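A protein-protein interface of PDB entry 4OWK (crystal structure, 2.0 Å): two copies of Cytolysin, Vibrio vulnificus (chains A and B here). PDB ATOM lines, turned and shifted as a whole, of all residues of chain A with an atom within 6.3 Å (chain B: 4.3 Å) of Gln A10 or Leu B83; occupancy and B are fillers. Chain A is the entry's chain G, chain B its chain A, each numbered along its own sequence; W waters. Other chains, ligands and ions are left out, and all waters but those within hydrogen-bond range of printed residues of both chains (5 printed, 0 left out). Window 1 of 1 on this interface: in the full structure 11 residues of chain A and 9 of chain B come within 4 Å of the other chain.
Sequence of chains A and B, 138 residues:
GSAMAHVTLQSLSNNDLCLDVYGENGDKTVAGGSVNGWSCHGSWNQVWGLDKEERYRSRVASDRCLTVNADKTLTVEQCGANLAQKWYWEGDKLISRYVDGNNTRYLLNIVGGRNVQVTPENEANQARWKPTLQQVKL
Of the 9 printed residues of chain B, 6 touch a printed residue of chain A. Along chain B the printed residues that touch a printed residue of chain A span positions 81 to 98. Printed residues of chain A that touch a printed residue of chain B: Gln A10, Ser A11, Leu A12, Asn A14, Asn A15, Asp A16, Cys A40 and Arg A128. Hydrophobic or aromatic side chains of chain A that line the printed part of chain B: Leu A12.
Gln A10 touches Leu B83. OE1 of Gln A10 touches CE of Lys B86 (3.98 Å). CD1 of Leu B83 touches O of Ser A11, at 3.8 Å. Leu B83 touches Leu A12 (CD1 to CA, 3.8 Å). CD of Arg B97 touches CD2 of Leu A12 (3.8 Å). Asn A14 touches Leu B83 (O to CD1, 3.3 Å). OD1 of Asn A15 touches CA of Tyr B98, at 3.6 Å. Asn B82 touches Asp A16 (ND2 to CB, 3.8 Å). Cys A40 touches Ala B81 (CB to CB, 3.8 Å). NH2 of Arg A128 touches NH1 of Arg B97, 3.99 Å away.
The backbone carbonyl oxygen (O) of Lys B86 sits at hydrogen-bond distance from the backbone NH (N) of Arg B97, at 2.9 Å. The backbone NH (N) of Lys A130 sits at hydrogen-bond distance from the backbone carbonyl oxygen (O) of Gln A10, at 2.7 Å. The side-chain hydroxyl (OG) of Ser A11 lies within hydrogen-bond range of the backbone NH (N) of Ser A13 (2.9 Å). N of Leu A12 is in hydrogen-bond range of O of Arg A128, at 2.8 Å. N of Arg A128 is in hydrogen-bond range of OG of Ser A13 (3.1 Å). N of Cys A40 sits at hydrogen-bond distance from OD1 of Asp A16.
Water W4 bridges the side-chain amino group (NZ) of Lys A130 (2.5 Å) and the side-chain amino group (NZ) of Lys B86 (3.3 Å). Water W3 bridges O of Leu A12 (2.7 Å) and O of Arg B97 (2.7 Å). Water W2 bridges OD2 of Asp A16 (2.8 Å) and ND2 of Asn B82 (2.9 Å). Water W5 lies within hydrogen-bond range of NZ of Lys B86 and OE1 of Gln A10. Water W1 lies within hydrogen-bond range of the guanidinium group of Arg B97 (2.9 Å) and the guanidinium group of Arg A128 (3.0 Å).
Printed residues of chain B within 4 Å of Cys A40: Ala B81. Of the printed residues of chain B, Arg A128 touches Arg B97. Of the printed residues of chain A, Tyr B98 touches Asn A15 (3.6 Å).
O of Ala B81 sits at hydrogen-bond distance from NE2 of Gln A10 (2.8 Å). The side-chain amide oxygen of Asn B82 lies close to the backbone carbonyl oxygen of Asn A15 (3.4 Å). The backbone NH (N) of Leu B83 lies within hydrogen-bond range of the backbone carbonyl oxygen (O) of Asn A15 (2.8 Å).
No position is printed for both chains. Of the 13 pairs that touch across the chains among the printed residues, none has its exchanged pair printed and touching as well.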
ATOM      1  N   THR A   8      24.829   7.176   7.933  1.00  0.00           N
ATOM      2  CA  THR A   8      24.502   6.002   7.133  1.00  0.00           C
ATOM      3  C   THR A   8      23.000   5.810   7.269  1.00  0.00           C
ATOM      4  O   THR A   8      22.392   6.183   8.286  1.00  0.00           O
ATOM      5  CB  THR A   8      25.274   4.735   7.574  1.00  0.00           C
ATOM      6  OG1 THR A   8      25.068   4.511   8.973  1.00  0.00           O
ATOM      7  CG2 THR A   8      26.752   4.889   7.295  1.00  0.00           C
ATOM      8  N   LEU A   9      22.377   5.284   6.231  1.00  0.00           N
ATOM      9  CA  LEU A   9      20.936   4.977   6.303  1.00  0.00           C
ATOM     10  C   LEU A   9      20.819   3.478   6.493  1.00  0.00           C
ATOM     11  O   LEU A   9      20.884   2.716   5.525  1.00  0.00           O
ATOM     12  CB  LEU A   9      20.203   5.435   5.042  1.00  0.00           C
ATOM     13  CG  LEU A   9      20.163   6.947   4.873  1.00  0.00           C
ATOM     14  CD1 LEU A   9      19.664   7.281   3.488  1.00  0.00           C
ATOM     15  CD2 LEU A   9      19.262   7.585   5.934  1.00  0.00           C
ATOM     16  N   GLN A  10      20.716   3.050   7.745  1.00  0.00           N
ATOM     17  CA  GLN A  10      20.738   1.617   8.029  1.00  0.00           C
ATOM     18  C   GLN A  10      19.324   1.099   8.239  1.00  0.00           C
ATOM     19  O   GLN A  10      18.502   1.719   8.947  1.00  0.00           O
ATOM     20  CB  GLN A  10      21.612   1.301   9.263  1.00  0.00           C
ATOM     21  CG  GLN A  10      21.718  -0.191   9.497  1.00  0.00           C
ATOM     22  CD  GLN A  10      22.716  -0.621  10.566  1.00  0.00           C
ATOM     23  OE1 GLN A  10      23.456   0.181  11.139  1.00  0.00           O
ATOM     24  NE2 GLN A  10      22.735  -1.911  10.828  1.00  0.00           N
ATOM     25  N   SER A  11      19.050  -0.058   7.655  1.00  0.00           N
ATOM     26  CA  SER A  11      17.757  -0.709   7.802  1.00  0.00           C
ATOM     27  C   SER A  11      17.563  -1.290   9.202  1.00  0.00           C
ATOM     28  O   SER A  11      18.501  -1.824   9.798  1.00  0.00           O
ATOM     29  CB  SER A  11      17.603  -1.818   6.758  1.00  0.00           C
ATOM     30  OG  SER A  11      16.417  -2.571   6.967  1.00  0.00           O
ATOM     31  N   LEU A  12      16.333  -1.200   9.701  1.00  0.00           N
ATOM     32  CA  LEU A  12      15.913  -1.927  10.903  1.00  0.00           C
ATOM     33  C   LEU A  12      15.008  -3.121  10.562  1.00  0.00           C
ATOM     34  O   LEU A  12      14.441  -3.770  11.450  1.00  0.00           O
ATOM     35  CB  LEU A  12      15.202  -0.975  11.875  1.00  0.00           C
ATOM     36  CG  LEU A  12      16.006   0.224  12.404  1.00  0.00           C
ATOM     37  CD1 LEU A  12      15.166   1.099  13.346  1.00  0.00           C
ATOM     38  CD2 LEU A  12      17.267  -0.254  13.142  1.00  0.00           C
ATOM     39  N   SER A  13      14.892  -3.426   9.273  1.00  0.00           N
ATOM     40  CA  SER A  13      14.072  -4.542   8.804  1.00  0.00           C
ATOM     41  C   SER A  13      14.944  -5.671   8.254  1.00  0.00           C
ATOM     42  O   SER A  13      14.446  -6.639   7.700  1.00  0.00           O
ATOM     43  CB  SER A  13      13.108  -4.082   7.708  1.00  0.00           C
ATOM     44  OG  SER A  13      12.326  -2.960   8.098  1.00  0.00           O
ATOM     45  N   ASN A  14      16.251  -5.527   8.400  1.00  0.00           N
ATOM     46  CA  ASN A  14      17.237  -6.490   7.881  1.00  0.00           C
ATOM     47  C   ASN A  14      18.464  -6.394   8.789  1.00  0.00           C
ATOM     48  O   ASN A  14      18.926  -5.283   9.090  1.00  0.00           O
ATOM     49  CB  ASN A  14      17.578  -6.150   6.423  1.00  0.00           C
ATOM     50  CG  ASN A  14      18.634  -7.067   5.822  1.00  0.00           C
ATOM     51  OD1 ASN A  14      19.752  -7.183   6.343  1.00  0.00           O
ATOM     52  ND2 ASN A  14      18.289  -7.701   4.695  1.00  0.00           N
ATOM     53  N   ASN A  15      19.009  -7.525   9.219  1.00  0.00           N
ATOM     54  CA  ASN A  15      20.042  -7.491  10.244  1.00  0.00           C
ATOM     55  C   ASN A  15      21.347  -6.798   9.864  1.00  0.00           C
ATOM     56  O   ASN A  15      22.133  -6.500  10.752  1.00  0.00           O
ATOM     57  CB  ASN A  15      20.345  -8.905  10.697  1.00  0.00           C
ATOM     58  CG  ASN A  15      19.177  -9.516  11.410  1.00  0.00           C
ATOM     59  OD1 ASN A  15      18.552  -8.870  12.248  1.00  0.00           O
ATOM     60  ND2 ASN A  15      18.824 -10.732  11.038  1.00  0.00           N
ATOM     61  N   ASP A  16      21.596  -6.572   8.571  1.00  0.00           N
ATOM     62  CA  ASP A  16      22.781  -5.806   8.149  1.00  0.00           C
ATOM     63  C   ASP A  16      22.596  -5.331   6.712  1.00  0.00           C
ATOM     64  O   ASP A  16      23.009  -6.001   5.756  1.00  0.00           O
ATOM     65  CB  ASP A  16      24.100  -6.624   8.269  1.00  0.00           C
ATOM     66  CG  ASP A  16      25.373  -5.764   7.984  1.00  0.00           C
ATOM     67  OD1 ASP A  16      25.247  -4.550   7.658  1.00  0.00           O
ATOM     68  OD2 ASP A  16      26.515  -6.308   8.052  1.00  0.00           O
ATOM     69  N   LEU A  17      21.960  -4.181   6.564  1.00  0.00           N
ATOM     70  CA  LEU A  17      21.777  -3.583   5.257  1.00  0.00           C
ATOM     71  C   LEU A  17      21.763  -2.070   5.418  1.00  0.00           C
ATOM     72  O   LEU A  17      21.016  -1.538   6.250  1.00  0.00           O
ATOM     73  CB  LEU A  17      20.484  -4.084   4.583  1.00  0.00           C
ATOM     74  CG  LEU A  17      20.265  -3.564   3.151  1.00  0.00           C
ATOM     75  CD1 LEU A  17      19.532  -4.563   2.298  1.00  0.00           C
ATOM     76  CD2 LEU A  17      19.503  -2.250   3.137  1.00  0.00           C
ATOM     77  N   CYS A  18      22.606  -1.405   4.622  1.00  0.00           N
ATOM     78  CA  CYS A  18      22.694   0.052   4.530  1.00  0.00           C
ATOM     79  C   CYS A  18      22.409   0.534   3.088  1.00  0.00           C
ATOM     80  O   CYS A  18      22.782  -0.129   2.121  1.00  0.00           O
ATOM     81  CB  CYS A  18      24.099   0.505   4.961  1.00  0.00           C
ATOM     82  SG  CYS A  18      24.298   0.530   6.785  1.00  0.00           S
ATOM     83  N   LEU A  19      21.804   1.697   2.930  1.00  0.00           N
ATOM     84  CA  LEU A  19      21.532   2.217   1.587  1.00  0.00           C
ATOM     85  C   LEU A  19      22.854   2.541   0.927  1.00  0.00           C
ATOM     86  O   LEU A  19      23.709   3.195   1.541  1.00  0.00           O
ATOM     87  CB  LEU A  19      20.644   3.448   1.641  1.00  0.00           C
ATOM     88  CG  LEU A  19      20.037   3.833   0.281  1.00  0.00           C
ATOM     89  CD1 LEU A  19      19.032   2.763  -0.150  1.00  0.00           C
ATOM     90  CD2 LEU A  19      19.365   5.224   0.400  1.00  0.00           C
ATOM     91  N   CYS A  40      26.799  -3.087   5.928  1.00  0.00           N
ATOM     92  CA  CYS A  40      27.271  -1.777   6.359  1.00  0.00           C
ATOM     93  C   CYS A  40      28.792  -1.706   6.526  1.00  0.00           C
ATOM     94  O   CYS A  40      29.373  -2.540   7.215  1.00  0.00           O
ATOM     95  CB  CYS A  40      26.596  -1.410   7.679  1.00  0.00           C
ATOM     96  SG  CYS A  40      24.796  -1.315   7.577  1.00  0.00           S
ATOM     97  N   ARG A 128      11.653   0.039   7.540  1.00  0.00           N
ATOM     98  CA  ARG A 128      12.164   0.725   8.731  1.00  0.00           C
ATOM     99  C   ARG A 128      13.646   1.057   8.561  1.00  0.00           C
ATOM    100  O   ARG A 128      14.447   0.188   8.181  1.00  0.00           O
ATOM    101  CB  ARG A 128      11.952  -0.126   9.977  1.00  0.00           C
ATOM    102  CG  ARG A 128      10.516  -0.582  10.180  1.00  0.00           C
ATOM    103  CD  ARG A 128      10.437  -1.509  11.384  1.00  0.00           C
ATOM    104  NE  ARG A 128      11.051  -0.910  12.568  1.00  0.00           N
ATOM    105  CZ  ARG A 128      11.549  -1.601  13.593  1.00  0.00           C
ATOM    106  NH1 ARG A 128      11.522  -2.933  13.597  1.00  0.00           N
ATOM    107  NH2 ARG A 128      12.097  -0.954  14.615  1.00  0.00           N
ATOM    108  N   TRP A 129      13.992   2.314   8.850  1.00  0.00           N
ATOM    109  CA  TRP A 129      15.359   2.840   8.696  1.00  0.00           C
ATOM    110  C   TRP A 129      15.788   3.656   9.900  1.00  0.00           C
ATOM    111  O   TRP A 129      14.948   4.237  10.617  1.00  0.00           O
ATOM    112  CB  TRP A 129      15.474   3.723   7.440  1.00  0.00           C
ATOM    113  CG  TRP A 129      15.067   2.992   6.220  1.00  0.00           C
ATOM    114  CD1 TRP A 129      13.803   2.886   5.726  1.00  0.00           C
ATOM    115  CD2 TRP A 129      15.905   2.199   5.364  1.00  0.00           C
ATOM    116  NE1 TRP A 129      13.791   2.066   4.627  1.00  0.00           N
ATOM    117  CE2 TRP A 129      15.071   1.644   4.368  1.00  0.00           C
ATOM    118  CE3 TRP A 129      17.269   1.900   5.341  1.00  0.00           C
ATOM    119  CZ2 TRP A 129      15.561   0.816   3.360  1.00  0.00           C
ATOM    120  CZ3 TRP A 129      17.759   1.073   4.330  1.00  0.00           C
ATOM    121  CH2 TRP A 129      16.903   0.530   3.367  1.00  0.00           C
ATOM    122  N   LYS A 130      17.099   3.708  10.111  1.00  0.00           N
ATOM    123  CA  LYS A 130      17.697   4.504  11.183  1.00  0.00           C
ATOM    124  C   LYS A 130      18.803   5.360  10.544  1.00  0.00           C
ATOM    125  O   LYS A 130      19.764   4.820   9.991  1.00  0.00           O
ATOM    126  CB  LYS A 130      18.260   3.613  12.296  1.00  0.00           C
ATOM    127  CG  LYS A 130      18.793   4.396  13.506  1.00  0.00           C
ATOM    128  CD  LYS A 130      19.777   3.568  14.347  1.00  0.00           C
ATOM    129  CE  LYS A 130      20.188   4.309  15.638  1.00  0.00           C
ATOM    130  NZ  LYS A 130      21.270   3.595  16.391  1.00  0.00           N
ATOM    131  N   PRO A 131      18.637   6.688  10.558  1.00  0.00           N
ATOM    132  CA  PRO A 131      19.719   7.567  10.108  1.00  0.00           C
ATOM    133  C   PRO A 131      20.785   7.595  11.197  1.00  0.00           C
ATOM    134  O   PRO A 131      20.535   8.112  12.279  1.00  0.00           O
ATOM    135  CB  PRO A 131      19.040   8.921   9.944  1.00  0.00           C
ATOM    136  CG  PRO A 131      17.904   8.882  10.944  1.00  0.00           C
ATOM    137  CD  PRO A 131      17.475   7.452  11.068  1.00  0.00           C
ATOM    138  N   THR A 132      21.937   7.006  10.923  1.00  0.00           N
ATOM    139  CA  THR A 132      22.949   6.756  11.946  1.00  0.00           C
ATOM    140  C   THR A 132      24.168   7.658  11.780  1.00  0.00           C
ATOM    141  O   THR A 132      24.883   7.548  10.786  1.00  0.00           O
ATOM    142  CB  THR A 132      23.420   5.298  11.882  1.00  0.00           C
ATOM    143  OG1 THR A 132      22.274   4.437  11.788  1.00  0.00           O
ATOM    144  CG2 THR A 132      24.248   4.954  13.102  1.00  0.00           C
ATOM    145  N   ALA B  81      28.008  -3.708  13.041  1.00  0.00           N
ATOM    146  CA  ALA B  81      26.774  -2.997  12.665  1.00  0.00           C
ATOM    147  C   ALA B  81      25.528  -3.871  12.717  1.00  0.00           C
ATOM    148  O   ALA B  81      24.418  -3.366  12.550  1.00  0.00           O
ATOM    149  CB  ALA B  81      26.909  -2.423  11.278  1.00  0.00           C
ATOM    150  N   ASN B  82      25.700  -5.174  12.919  1.00  0.00           N
ATOM    151  CA  ASN B  82      24.569  -6.088  12.847  1.00  0.00           C
ATOM    152  C   ASN B  82      23.489  -5.752  13.898  1.00  0.00           C
ATOM    153  O   ASN B  82      23.813  -5.339  15.018  1.00  0.00           O
ATOM    154  CB  ASN B  82      25.038  -7.535  13.024  1.00  0.00           C
ATOM    155  CG  ASN B  82      24.062  -8.528  12.437  1.00  0.00           C
ATOM    156  OD1 ASN B  82      23.026  -8.822  13.034  1.00  0.00           O
ATOM    157  ND2 ASN B  82      24.377  -9.034  11.233  1.00  0.00           N
ATOM    158  N   LEU B  83      22.217  -5.893  13.525  1.00  0.00           N
ATOM    159  CA  LEU B  83      21.133  -5.641  14.459  1.00  0.00           C
ATOM    160  C   LEU B  83      21.171  -6.602  15.656  1.00  0.00           C
ATOM    161  O   LEU B  83      20.585  -6.329  16.698  1.00  0.00           O
ATOM    162  CB  LEU B  83      19.784  -5.744  13.759  1.00  0.00           C
ATOM    163  CG  LEU B  83      19.508  -4.713  12.655  1.00  0.00           C
ATOM    164  CD1 LEU B  83      18.057  -4.778  12.182  1.00  0.00           C
ATOM    165  CD2 LEU B  83      19.882  -3.298  13.095  1.00  0.00           C
ATOM    166  N   ALA B  84      21.860  -7.724  15.501  1.00  0.00           N
ATOM    167  CA  ALA B  84      21.998  -8.716  16.587  1.00  0.00           C
ATOM    168  C   ALA B  84      22.809  -8.182  17.750  1.00  0.00           C
ATOM    169  O   ALA B  84      22.856  -8.798  18.833  1.00  0.00           O
ATOM    170  CB  ALA B  84      22.643 -10.013  16.061  1.00  0.00           C
ATOM    171  N   GLN B  85      23.432  -7.032  17.549  1.00  0.00           N
ATOM    172  CA  GLN B  85      24.145  -6.367  18.638  1.00  0.00           C
ATOM    173  C   GLN B  85      23.423  -5.110  19.138  1.00  0.00           C
ATOM    174  O   GLN B  85      23.943  -4.377  19.986  1.00  0.00           O
ATOM    175  CB  GLN B  85      25.561  -6.021  18.172  1.00  0.00           C
ATOM    176  CG  GLN B  85      26.428  -7.273  17.905  1.00  0.00           C
ATOM    177  CD  GLN B  85      27.873  -6.932  17.598  1.00  0.00           C
ATOM    178  OE1 GLN B  85      28.166  -5.904  16.993  1.00  0.00           O
ATOM    179  NE2 GLN B  85      28.783  -7.788  18.029  1.00  0.00           N
ATOM    180  N   LYS B  86      22.228  -4.850  18.621  1.00  0.00           N
ATOM    181  CA  LYS B  86      21.529  -3.634  19.033  1.00  0.00           C
ATOM    182  C   LYS B  86      20.370  -3.919  19.992  1.00  0.00           C
ATOM    183  O   LYS B  86      19.624  -4.873  19.826  1.00  0.00           O
ATOM    184  CB  LYS B  86      21.044  -2.865  17.817  1.00  0.00           C
ATOM    185  CG  LYS B  86      22.172  -2.343  16.956  1.00  0.00           C
ATOM    186  CD  LYS B  86      21.656  -1.348  15.923  1.00  0.00           C
ATOM    187  CE  LYS B  86      22.640  -1.147  14.800  1.00  0.00           C
ATOM    188  NZ  LYS B  86      23.954  -0.819  15.354  1.00  0.00           N
ATOM    189  N   SER B  96      15.886  -6.840  21.718  1.00  0.00           N
ATOM    190  CA  SER B  96      16.869  -6.929  20.643  1.00  0.00           C
ATOM    191  C   SER B  96      16.310  -6.369  19.327  1.00  0.00           C
ATOM    192  O   SER B  96      15.119  -6.493  19.071  1.00  0.00           O
ATOM    193  CB  SER B  96      17.282  -8.388  20.454  1.00  0.00           C
ATOM    194  OG  SER B  96      18.126  -8.561  19.329  1.00  0.00           O
ATOM    195  N   ARG B  97      17.154  -5.759  18.490  1.00  0.00           N
ATOM    196  CA  ARG B  97      16.673  -5.308  17.189  1.00  0.00           C
ATOM    197  C   ARG B  97      16.771  -6.434  16.152  1.00  0.00           C
ATOM    198  O   ARG B  97      16.454  -6.222  14.986  1.00  0.00           O
ATOM    199  CB  ARG B  97      17.451  -4.074  16.716  1.00  0.00           C
ATOM    200  CG  ARG B  97      17.160  -2.829  17.538  1.00  0.00           C
ATOM    201  CD  ARG B  97      17.247  -1.572  16.690  1.00  0.00           C
ATOM    202  NE  ARG B  97      17.120  -0.361  17.499  1.00  0.00           N
ATOM    203  CZ  ARG B  97      15.959   0.179  17.853  1.00  0.00           C
ATOM    204  NH1 ARG B  97      14.815  -0.401  17.490  1.00  0.00           N
ATOM    205  NH2 ARG B  97      15.943   1.299  18.577  1.00  0.00           N
ATOM    206  N   TYR B  98      17.229  -7.613  16.580  1.00  0.00           N
ATOM    207  CA  TYR B  98      17.375  -8.779  15.684  1.00  0.00           C
ATOM    208  C   TYR B  98      16.074  -9.084  14.967  1.00  0.00           C
ATOM    209  O   TYR B  98      15.034  -9.115  15.598  1.00  0.00           O
ATOM    210  CB  TYR B  98      17.828 -10.024  16.477  1.00  0.00           C
ATOM    211  CG  TYR B  98      17.841 -11.310  15.650  1.00  0.00           C
ATOM    212  CD1 TYR B  98      18.948 -11.656  14.868  1.00  0.00           C
ATOM    213  CD2 TYR B  98      16.745 -12.167  15.635  1.00  0.00           C
ATOM    214  CE1 TYR B  98      18.961 -12.825  14.102  1.00  0.00           C
ATOM    215  CE2 TYR B  98      16.755 -13.339  14.872  1.00  0.00           C
ATOM    216  CZ  TYR B  98      17.862 -13.653  14.107  1.00  0.00           C
ATOM    217  OH  TYR B  98      17.872 -14.802  13.347  1.00  0.00           O
HETATM  218  O   HOH W   1      13.802  -2.845  16.199  1.00  0.00           O
HETATM  219  O   HOH W   2      26.876  -8.058  10.257  1.00  0.00           O
HETATM  220  O   HOH W   3      14.876  -4.188  14.067  1.00  0.00           O
HETATM  221  O   HOH W   4      23.190   2.388  15.344  1.00  0.00           O
HETATM  222  O   HOH W   5      25.562   0.251  13.263  1.00  0.00           O
